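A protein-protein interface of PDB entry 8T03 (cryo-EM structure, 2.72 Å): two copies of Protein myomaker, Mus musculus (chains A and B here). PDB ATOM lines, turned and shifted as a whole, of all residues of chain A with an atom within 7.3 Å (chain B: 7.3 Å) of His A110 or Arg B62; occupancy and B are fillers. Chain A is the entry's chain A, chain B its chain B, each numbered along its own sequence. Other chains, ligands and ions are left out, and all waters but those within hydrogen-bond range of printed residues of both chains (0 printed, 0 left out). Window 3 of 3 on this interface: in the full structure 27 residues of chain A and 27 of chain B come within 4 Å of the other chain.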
ATOM      1  N   TYR A  68      11.645   6.949  -6.151  1.00  0.00           N
ATOM      2  CA  TYR A  68      12.008   8.145  -5.344  1.00  0.00           C
ATOM      3  C   TYR A  68      13.021   9.006  -6.114  1.00  0.00           C
ATOM      4  O   TYR A  68      12.770  10.221  -6.247  1.00  0.00           O
ATOM      5  CB  TYR A  68      12.546   7.767  -3.960  1.00  0.00           C
ATOM      6  CG  TYR A  68      12.981   8.964  -3.153  1.00  0.00           C
ATOM      7  CD1 TYR A  68      12.053   9.770  -2.514  1.00  0.00           C
ATOM      8  CD2 TYR A  68      14.317   9.329  -3.077  1.00  0.00           C
ATOM      9  CE1 TYR A  68      12.442  10.889  -1.795  1.00  0.00           C
ATOM     10  CE2 TYR A  68      14.722  10.447  -2.362  1.00  0.00           C
ATOM     11  CZ  TYR A  68      13.781  11.230  -1.717  1.00  0.00           C
ATOM     12  OH  TYR A  68      14.173  12.329  -1.009  1.00  0.00           O
ATOM     13  N   ILE A 104      13.863  20.022  -1.656  1.00  0.00           N
ATOM     14  CA  ILE A 104      13.294  19.017  -2.609  1.00  0.00           C
ATOM     15  C   ILE A 104      13.404  17.622  -1.975  1.00  0.00           C
ATOM     16  O   ILE A 104      12.469  16.823  -2.173  1.00  0.00           O
ATOM     17  CB  ILE A 104      13.949  19.096  -4.009  1.00  0.00           C
ATOM     18  CG1 ILE A 104      13.665  20.448  -4.672  1.00  0.00           C
ATOM     19  CG2 ILE A 104      13.492  17.950  -4.906  1.00  0.00           C
ATOM     20  CD1 ILE A 104      14.520  20.751  -5.884  1.00  0.00           C
ATOM     21  N   ALA A 105      14.483  17.346  -1.230  1.00  0.00           N
ATOM     22  CA  ALA A 105      14.721  16.053  -0.542  1.00  0.00           C
ATOM     23  C   ALA A 105      13.621  15.811   0.498  1.00  0.00           C
ATOM     24  O   ALA A 105      12.981  14.744   0.424  1.00  0.00           O
ATOM     25  CB  ALA A 105      16.095  16.019   0.084  1.00  0.00           C
ATOM     26  N   VAL A 106      13.396  16.769   1.407  1.00  0.00           N
ATOM     27  CA  VAL A 106      12.400  16.657   2.518  1.00  0.00           C
ATOM     28  C   VAL A 106      10.991  16.590   1.921  1.00  0.00           C
ATOM     29  O   VAL A 106      10.211  15.732   2.382  1.00  0.00           O
ATOM     30  CB  VAL A 106      12.513  17.799   3.549  1.00  0.00           C
ATOM     31  CG1 VAL A 106      11.383  17.759   4.573  1.00  0.00           C
ATOM     32  CG2 VAL A 106      13.855  17.776   4.260  1.00  0.00           C
ATOM     33  N   ARG A 107      10.671  17.468   0.964  1.00  0.00           N
ATOM     34  CA  ARG A 107       9.321  17.506   0.342  1.00  0.00           C
ATOM     35  C   ARG A 107       9.040  16.159  -0.342  1.00  0.00           C
ATOM     36  O   ARG A 107       7.980  15.574  -0.042  1.00  0.00           O
ATOM     37  CB  ARG A 107       9.171  18.674  -0.639  1.00  0.00           C
ATOM     38  CG  ARG A 107       7.977  18.533  -1.575  1.00  0.00           C
ATOM     39  CD  ARG A 107       6.716  19.130  -0.986  1.00  0.00           C
ATOM     40  NE  ARG A 107       5.497  18.472  -1.444  1.00  0.00           N
ATOM     41  CZ  ARG A 107       4.722  17.663  -0.717  1.00  0.00           C
ATOM     42  NH1 ARG A 107       5.009  17.372   0.541  1.00  0.00           N
ATOM     43  NH2 ARG A 107       3.637  17.141  -1.262  1.00  0.00           N
ATOM     44  N   THR A 108       9.925  15.700  -1.239  1.00  0.00           N
ATOM     45  CA  THR A 108       9.746  14.436  -2.013  1.00  0.00           C
ATOM     46  C   THR A 108       9.625  13.245  -1.053  1.00  0.00           C
ATOM     47  O   THR A 108       8.797  12.358  -1.336  1.00  0.00           O
ATOM     48  CB  THR A 108      10.864  14.189  -3.037  1.00  0.00           C
ATOM     49  OG1 THR A 108      11.066  15.389  -3.784  1.00  0.00           O
ATOM     50  CG2 THR A 108      10.545  13.058  -3.993  1.00  0.00           C
ATOM     51  N   PHE A 109      10.408  13.225   0.031  1.00  0.00           N
ATOM     52  CA  PHE A 109      10.425  12.127   1.035  1.00  0.00           C
ATOM     53  C   PHE A 109       9.113  12.134   1.831  1.00  0.00           C
ATOM     54  O   PHE A 109       8.642  11.034   2.186  1.00  0.00           O
ATOM     55  CB  PHE A 109      11.653  12.228   1.943  1.00  0.00           C
ATOM     56  CG  PHE A 109      11.934  10.986   2.753  1.00  0.00           C
ATOM     57  CD1 PHE A 109      11.247  10.738   3.930  1.00  0.00           C
ATOM     58  CD2 PHE A 109      12.886  10.065   2.338  1.00  0.00           C
ATOM     59  CE1 PHE A 109      11.498   9.595   4.675  1.00  0.00           C
ATOM     60  CE2 PHE A 109      13.141   8.924   3.086  1.00  0.00           C
ATOM     61  CZ  PHE A 109      12.447   8.691   4.252  1.00  0.00           C
ATOM     62  N   HIS A 110       8.542  13.316   2.100  1.00  0.00           N
ATOM     63  CA  HIS A 110       7.224  13.471   2.775  1.00  0.00           C
ATOM     64  C   HIS A 110       6.123  12.873   1.891  1.00  0.00           C
ATOM     65  O   HIS A 110       5.385  12.000   2.385  1.00  0.00           O
ATOM     66  CB  HIS A 110       6.919  14.932   3.133  1.00  0.00           C
ATOM     67  CG  HIS A 110       5.530  15.108   3.650  1.00  0.00           C
ATOM     68  ND1 HIS A 110       4.481  15.475   2.835  1.00  0.00           N
ATOM     69  CD2 HIS A 110       5.002  14.907   4.876  1.00  0.00           C
ATOM     70  CE1 HIS A 110       3.371  15.530   3.540  1.00  0.00           C
ATOM     71  NE2 HIS A 110       3.663  15.184   4.798  1.00  0.00           N
ATOM     72  N   ASP A 111       6.007  13.344   0.647  1.00  0.00           N
ATOM     73  CA  ASP A 111       5.044  12.810  -0.354  1.00  0.00           C
ATOM     74  C   ASP A 111       5.579  13.099  -1.759  1.00  0.00           C
ATOM     75  O   ASP A 111       5.559  14.275  -2.177  1.00  0.00           O
ATOM     76  CB  ASP A 111       3.639  13.383  -0.141  1.00  0.00           C
ATOM     77  CG  ASP A 111       2.551  12.742  -0.990  1.00  0.00           C
ATOM     78  OD1 ASP A 111       2.837  11.735  -1.672  1.00  0.00           O
ATOM     79  OD2 ASP A 111       1.415  13.254  -0.956  1.00  0.00           O
ATOM     80  N   ARG A 112       6.031  12.052  -2.452  1.00  0.00           N
ATOM     81  CA  ARG A 112       6.638  12.142  -3.805  1.00  0.00           C
ATOM     82  C   ARG A 112       5.547  12.368  -4.867  1.00  0.00           C
ATOM     83  O   ARG A 112       5.912  12.803  -5.979  1.00  0.00           O
ATOM     84  CB  ARG A 112       7.483  10.894  -4.078  1.00  0.00           C
ATOM     85  CG  ARG A 112       6.680   9.621  -4.304  1.00  0.00           C
ATOM     86  CD  ARG A 112       7.564   8.393  -4.281  1.00  0.00           C
ATOM     87  NE  ARG A 112       8.108   8.113  -2.957  1.00  0.00           N
ATOM     88  CZ  ARG A 112       8.774   7.011  -2.615  1.00  0.00           C
ATOM     89  NH1 ARG A 112       8.989   6.046  -3.497  1.00  0.00           N
ATOM     90  NH2 ARG A 112       9.222   6.877  -1.377  1.00  0.00           N
ATOM     91  N   TRP A 113       4.275  12.090  -4.548  1.00  0.00           N
ATOM     92  CA  TRP A 113       3.104  12.256  -5.456  1.00  0.00           C
ATOM     93  C   TRP A 113       2.250  13.469  -5.063  1.00  0.00           C
ATOM     94  O   TRP A 113       1.197  13.657  -5.699  1.00  0.00           O
ATOM     95  CB  TRP A 113       2.248  10.985  -5.461  1.00  0.00           C
ATOM     96  CG  TRP A 113       2.991   9.753  -5.872  1.00  0.00           C
ATOM     97  CD1 TRP A 113       3.234   8.651  -5.105  1.00  0.00           C
ATOM     98  CD2 TRP A 113       3.597   9.498  -7.150  1.00  0.00           C
ATOM     99  NE1 TRP A 113       3.946   7.726  -5.818  1.00  0.00           N
ATOM    100  CE2 TRP A 113       4.184   8.216  -7.076  1.00  0.00           C
ATOM    101  CE3 TRP A 113       3.701  10.220  -8.348  1.00  0.00           C
ATOM    102  CZ2 TRP A 113       4.864   7.646  -8.154  1.00  0.00           C
ATOM    103  CZ3 TRP A 113       4.372   9.655  -9.411  1.00  0.00           C
ATOM    104  CH2 TRP A 113       4.945   8.385  -9.313  1.00  0.00           C
ATOM    105  N   GLY A 114       2.662  14.255  -4.063  1.00  0.00           N
ATOM    106  CA  GLY A 114       1.883  15.403  -3.561  1.00  0.00           C
ATOM    107  C   GLY A 114       2.102  16.652  -4.400  1.00  0.00           C
ATOM    108  O   GLY A 114       3.009  16.642  -5.258  1.00  0.00           O
ATOM    109  N   CYS B  50      11.206  13.542  19.318  1.00  0.00           N
ATOM    110  CA  CYS B  50      10.131  12.638  18.820  1.00  0.00           C
ATOM    111  C   CYS B  50      10.284  11.224  19.402  1.00  0.00           C
ATOM    112  O   CYS B  50       9.256  10.520  19.483  1.00  0.00           O
ATOM    113  CB  CYS B  50      10.109  12.595  17.295  1.00  0.00           C
ATOM    114  SG  CYS B  50       8.566  11.932  16.609  1.00  0.00           S
ATOM    115  N   CYS B  59       6.441  16.241  17.881  1.00  0.00           N
ATOM    116  CA  CYS B  59       6.890  16.071  16.469  1.00  0.00           C
ATOM    117  C   CYS B  59       5.692  16.109  15.511  1.00  0.00           C
ATOM    118  O   CYS B  59       4.705  15.380  15.737  1.00  0.00           O
ATOM    119  CB  CYS B  59       7.750  14.828  16.257  1.00  0.00           C
ATOM    120  SG  CYS B  59       7.139  13.320  17.056  1.00  0.00           S
ATOM    121  N   PHE B  60       5.819  16.946  14.477  1.00  0.00           N
ATOM    122  CA  PHE B  60       4.772  17.354  13.500  1.00  0.00           C
ATOM    123  C   PHE B  60       4.859  16.477  12.246  1.00  0.00           C
ATOM    124  O   PHE B  60       3.865  16.428  11.487  1.00  0.00           O
ATOM    125  CB  PHE B  60       4.916  18.841  13.150  1.00  0.00           C
ATOM    126  CG  PHE B  60       6.249  19.235  12.559  1.00  0.00           C
ATOM    127  CD1 PHE B  60       7.343  19.490  13.375  1.00  0.00           C
ATOM    128  CD2 PHE B  60       6.413  19.349  11.185  1.00  0.00           C
ATOM    129  CE1 PHE B  60       8.572  19.837  12.832  1.00  0.00           C
ATOM    130  CE2 PHE B  60       7.642  19.702  10.644  1.00  0.00           C
ATOM    131  CZ  PHE B  60       8.718  19.946  11.467  1.00  0.00           C
ATOM    132  N   MET B  61       6.010  15.826  12.035  1.00  0.00           N
ATOM    133  CA  MET B  61       6.228  14.824  10.963  1.00  0.00           C
ATOM    134  C   MET B  61       6.518  13.467  11.604  1.00  0.00           C
ATOM    135  O   MET B  61       6.823  13.414  12.814  1.00  0.00           O
ATOM    136  CB  MET B  61       7.389  15.229  10.050  1.00  0.00           C
ATOM    137  CG  MET B  61       7.026  16.362   9.117  1.00  0.00           C
ATOM    138  SD  MET B  61       8.222  16.601   7.782  1.00  0.00           S
ATOM    139  CE  MET B  61       9.671  17.076   8.722  1.00  0.00           C
ATOM    140  N   ARG B  62       6.428  12.425  10.786  1.00  0.00           N
ATOM    141  CA  ARG B  62       6.513  11.004  11.208  1.00  0.00           C
ATOM    142  C   ARG B  62       7.973  10.665  11.506  1.00  0.00           C
ATOM    143  O   ARG B  62       8.870  11.384  11.017  1.00  0.00           O
ATOM    144  CB  ARG B  62       5.924  10.078  10.139  1.00  0.00           C
ATOM    145  CG  ARG B  62       6.087  10.595   8.719  1.00  0.00           C
ATOM    146  CD  ARG B  62       5.690   9.592   7.674  1.00  0.00           C
ATOM    147  NE  ARG B  62       5.848  10.180   6.357  1.00  0.00           N
ATOM    148  CZ  ARG B  62       5.862   9.511   5.211  1.00  0.00           C
ATOM    149  NH1 ARG B  62       5.730   8.194   5.193  1.00  0.00           N
ATOM    150  NH2 ARG B  62       6.016  10.172   4.077  1.00  0.00           N
ATOM    151  N   ARG B  63       8.179   9.602  12.284  1.00  0.00           N
ATOM    152  CA  ARG B  63       9.509   9.145  12.763  1.00  0.00           C
ATOM    153  C   ARG B  63      10.429   8.836  11.576  1.00  0.00           C
ATOM    154  O   ARG B  63      11.622   9.181  11.661  1.00  0.00           O
ATOM    155  CB  ARG B  63       9.341   7.918  13.660  1.00  0.00           C
ATOM    156  CG  ARG B  63       8.971   8.259  15.097  1.00  0.00           C
ATOM    157  CD  ARG B  63       9.696   7.391  16.111  1.00  0.00           C
ATOM    158  NE  ARG B  63      11.070   7.103  15.712  1.00  0.00           N
ATOM    159  CZ  ARG B  63      12.091   7.963  15.734  1.00  0.00           C
ATOM    160  NH1 ARG B  63      11.934   9.206  16.163  1.00  0.00           N
ATOM    161  NH2 ARG B  63      13.285   7.566  15.322  1.00  0.00           N
ATOM    162  N   ASP B  64       9.883   8.220  10.522  1.00  0.00           N
ATOM    163  CA  ASP B  64      10.608   7.792   9.293  1.00  0.00           C
ATOM    164  C   ASP B  64      11.331   8.983   8.647  1.00  0.00           C
ATOM    165  O   ASP B  64      12.477   8.787   8.193  1.00  0.00           O
ATOM    166  CB  ASP B  64       9.641   7.127   8.309  1.00  0.00           C
ATOM    167  CG  ASP B  64      10.296   6.579   7.050  1.00  0.00           C
ATOM    168  OD1 ASP B  64      11.450   6.110   7.139  1.00  0.00           O
ATOM    169  OD2 ASP B  64       9.642   6.622   5.989  1.00  0.00           O
ATOM    170  N   ILE B  65      10.699  10.164   8.606  1.00  0.00           N
ATOM    171  CA  ILE B  65      11.261  11.394   7.965  1.00  0.00           C
ATOM    172  C   ILE B  65      12.384  11.938   8.857  1.00  0.00           C
ATOM    173  O   ILE B  65      13.493  12.159   8.332  1.00  0.00           O
ATOM    174  CB  ILE B  65      10.177  12.459   7.684  1.00  0.00           C
ATOM    175  CG1 ILE B  65       9.026  11.893   6.845  1.00  0.00           C
ATOM    176  CG2 ILE B  65      10.796  13.694   7.033  1.00  0.00           C
ATOM    177  CD1 ILE B  65       7.960  12.903   6.462  1.00  0.00           C
ATOM    178  N   LEU B  66      12.101  12.138  10.150  1.00  0.00           N
ATOM    179  CA  LEU B  66      13.038  12.749  11.136  1.00  0.00           C
ATOM    180  C   LEU B  66      14.275  11.859  11.296  1.00  0.00           C
ATOM    181  O   LEU B  66      15.390  12.410  11.368  1.00  0.00           O
ATOM    182  CB  LEU B  66      12.324  12.934  12.481  1.00  0.00           C
ATOM    183  CG  LEU B  66      11.110  13.865  12.483  1.00  0.00           C
ATOM    184  CD1 LEU B  66      10.460  13.887  13.857  1.00  0.00           C
ATOM    185  CD2 LEU B  66      11.483  15.278  12.056  1.00  0.00           C
ATOM    186  N   GLU B  67      14.069  10.539  11.350  1.00  0.00           N
ATOM    187  CA  GLU B  67      15.130   9.499  11.448  1.00  0.00           C
ATOM    188  C   GLU B  67      16.024   9.543  10.203  1.00  0.00           C
ATOM    189  O   GLU B  67      17.258   9.494  10.374  1.00  0.00           O
ATOM    190  CB  GLU B  67      14.479   8.124  11.619  1.00  0.00           C
ATOM    191  CG  GLU B  67      15.451   6.965  11.732  1.00  0.00           C
ATOM    192  CD  GLU B  67      14.758   5.632  11.949  1.00  0.00           C
ATOM    193  OE1 GLU B  67      14.412   5.329  13.108  1.00  0.00           O
ATOM    194  OE2 GLU B  67      14.543   4.908  10.957  1.00  0.00           O
ATOM    195  N   TYR B  68      15.428   9.613   9.006  1.00  0.00           N
ATOM    196  CA  TYR B  68      16.160   9.633   7.711  1.00  0.00           C
ATOM    197  C   TYR B  68      17.050  10.883   7.634  1.00  0.00           C
ATOM    198  O   TYR B  68      18.252  10.723   7.343  1.00  0.00           O
ATOM    199  CB  TYR B  68      15.213   9.555   6.510  1.00  0.00           C
ATOM    200  CG  TYR B  68      15.934   9.640   5.188  1.00  0.00           C
ATOM    201  CD1 TYR B  68      16.600   8.543   4.667  1.00  0.00           C
ATOM    202  CD2 TYR B  68      16.004  10.834   4.486  1.00  0.00           C
ATOM    203  CE1 TYR B  68      17.291   8.620   3.467  1.00  0.00           C
ATOM    204  CE2 TYR B  68      16.691  10.928   3.285  1.00  0.00           C
ATOM    205  CZ  TYR B  68      17.336   9.817   2.773  1.00  0.00           C
ATOM    206  OH  TYR B  68      18.012   9.901   1.590  1.00  0.00           O
ATOM    207  N   PHE B  69      16.491  12.073   7.886  1.00  0.00           N
ATOM    208  CA  PHE B  69      17.183  13.379   7.690  1.00  0.00           C
ATOM    209  C   PHE B  69      18.086  13.716   8.884  1.00  0.00           C
ATOM    210  O   PHE B  69      18.931  14.621   8.735  1.00  0.00           O
ATOM    211  CB  PHE B  69      16.183  14.491   7.371  1.00  0.00           C
ATOM    212  CG  PHE B  69      15.625  14.367   5.980  1.00  0.00           C
ATOM    213  CD1 PHE B  69      16.456  14.507   4.878  1.00  0.00           C
ATOM    214  CD2 PHE B  69      14.292  14.046   5.767  1.00  0.00           C
ATOM    215  CE1 PHE B  69      15.960  14.363   3.592  1.00  0.00           C
ATOM    216  CE2 PHE B  69      13.798  13.899   4.481  1.00  0.00           C
ATOM    217  CZ  PHE B  69      14.633  14.058   3.396  1.00  0.00           C
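The backbone carbonyl oxygen (O) of Phe A109 sits at hydrogen-bond distance from the guanidinium group (NH2) of Arg B62 (3.3 Å). The backbone carbonyl oxygen (O) of His A110 sits at hydrogen-bond distance from the guanidinium group (NH2) of Arg B62 (2.6 Å).
OH of Tyr A68 lies within hydrogen-bond range of O of Ala A105, at 3.1 Å. NH1 of Arg A107 lies within hydrogen-bond range of ND1 of His A110 (3.0 Å). SG of Cys B59 is disulfide-bonded to SG of Cys B50.
Among the printed residues, pairs that only touch across the chains: Ala A105 with Phe B69 (3.5 Å), Val A106 with Phe B69 (3.5 Å), Phe A109 with Tyr B68 (3.6 Å), Phe A109 with Phe B69 (3.7 Å), Phe A109 with Asp B64 (3.7 Å), Phe A109 with Ile B65 (3.8 Å) and His A110 with Ile B65 (3.8 Å).
Printed residues of chain B within 4 Å of Ala A105: Phe B69. Of the printed residues of chain B, Val A106 touches Phe B69 (3.5 Å). Of the printed residues of chain B, Phe A109 touches Arg B62, Asp B64, Ile B65, Tyr B68 and Phe B69. Of the printed residues of chain B, His A110 touches Arg B62 and Ile B65. Gly A114 touches none of the printed residues of chain B. Printed residues of chain A within 4 Å of Arg B62: Phe A109 and His A110. Of the printed residues of chain A, Tyr B68 touches Phe A109. Printed residues of chain A within 4 Å of Phe B69: Ala A105, Val A106 and Phe A109. The nearest residue of chain B that does not touch His A110 is Met B61 (4.7 Å). The nearest printed residue of chain B that does not touch Phe A109 is Leu B66 (6.1 Å).
Printed residues of chain A that touch a printed residue of chain B: Ala A105, Val A106, Phe A109 and His A110. Hydrophobic or aromatic side chains of chain A within 4 Å of the printed part of chain B: Ala A105, Val A106, Phe A109 and His A110. Along chain A the printed residues that touch a printed residue of chain B span positions 105 to 110. Printed residues of chain B that touch a printed residue of chain A: Arg B62, Asp B64, Ile B65, Tyr B68 and Phe B69.
Position printed for both chains: 68.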
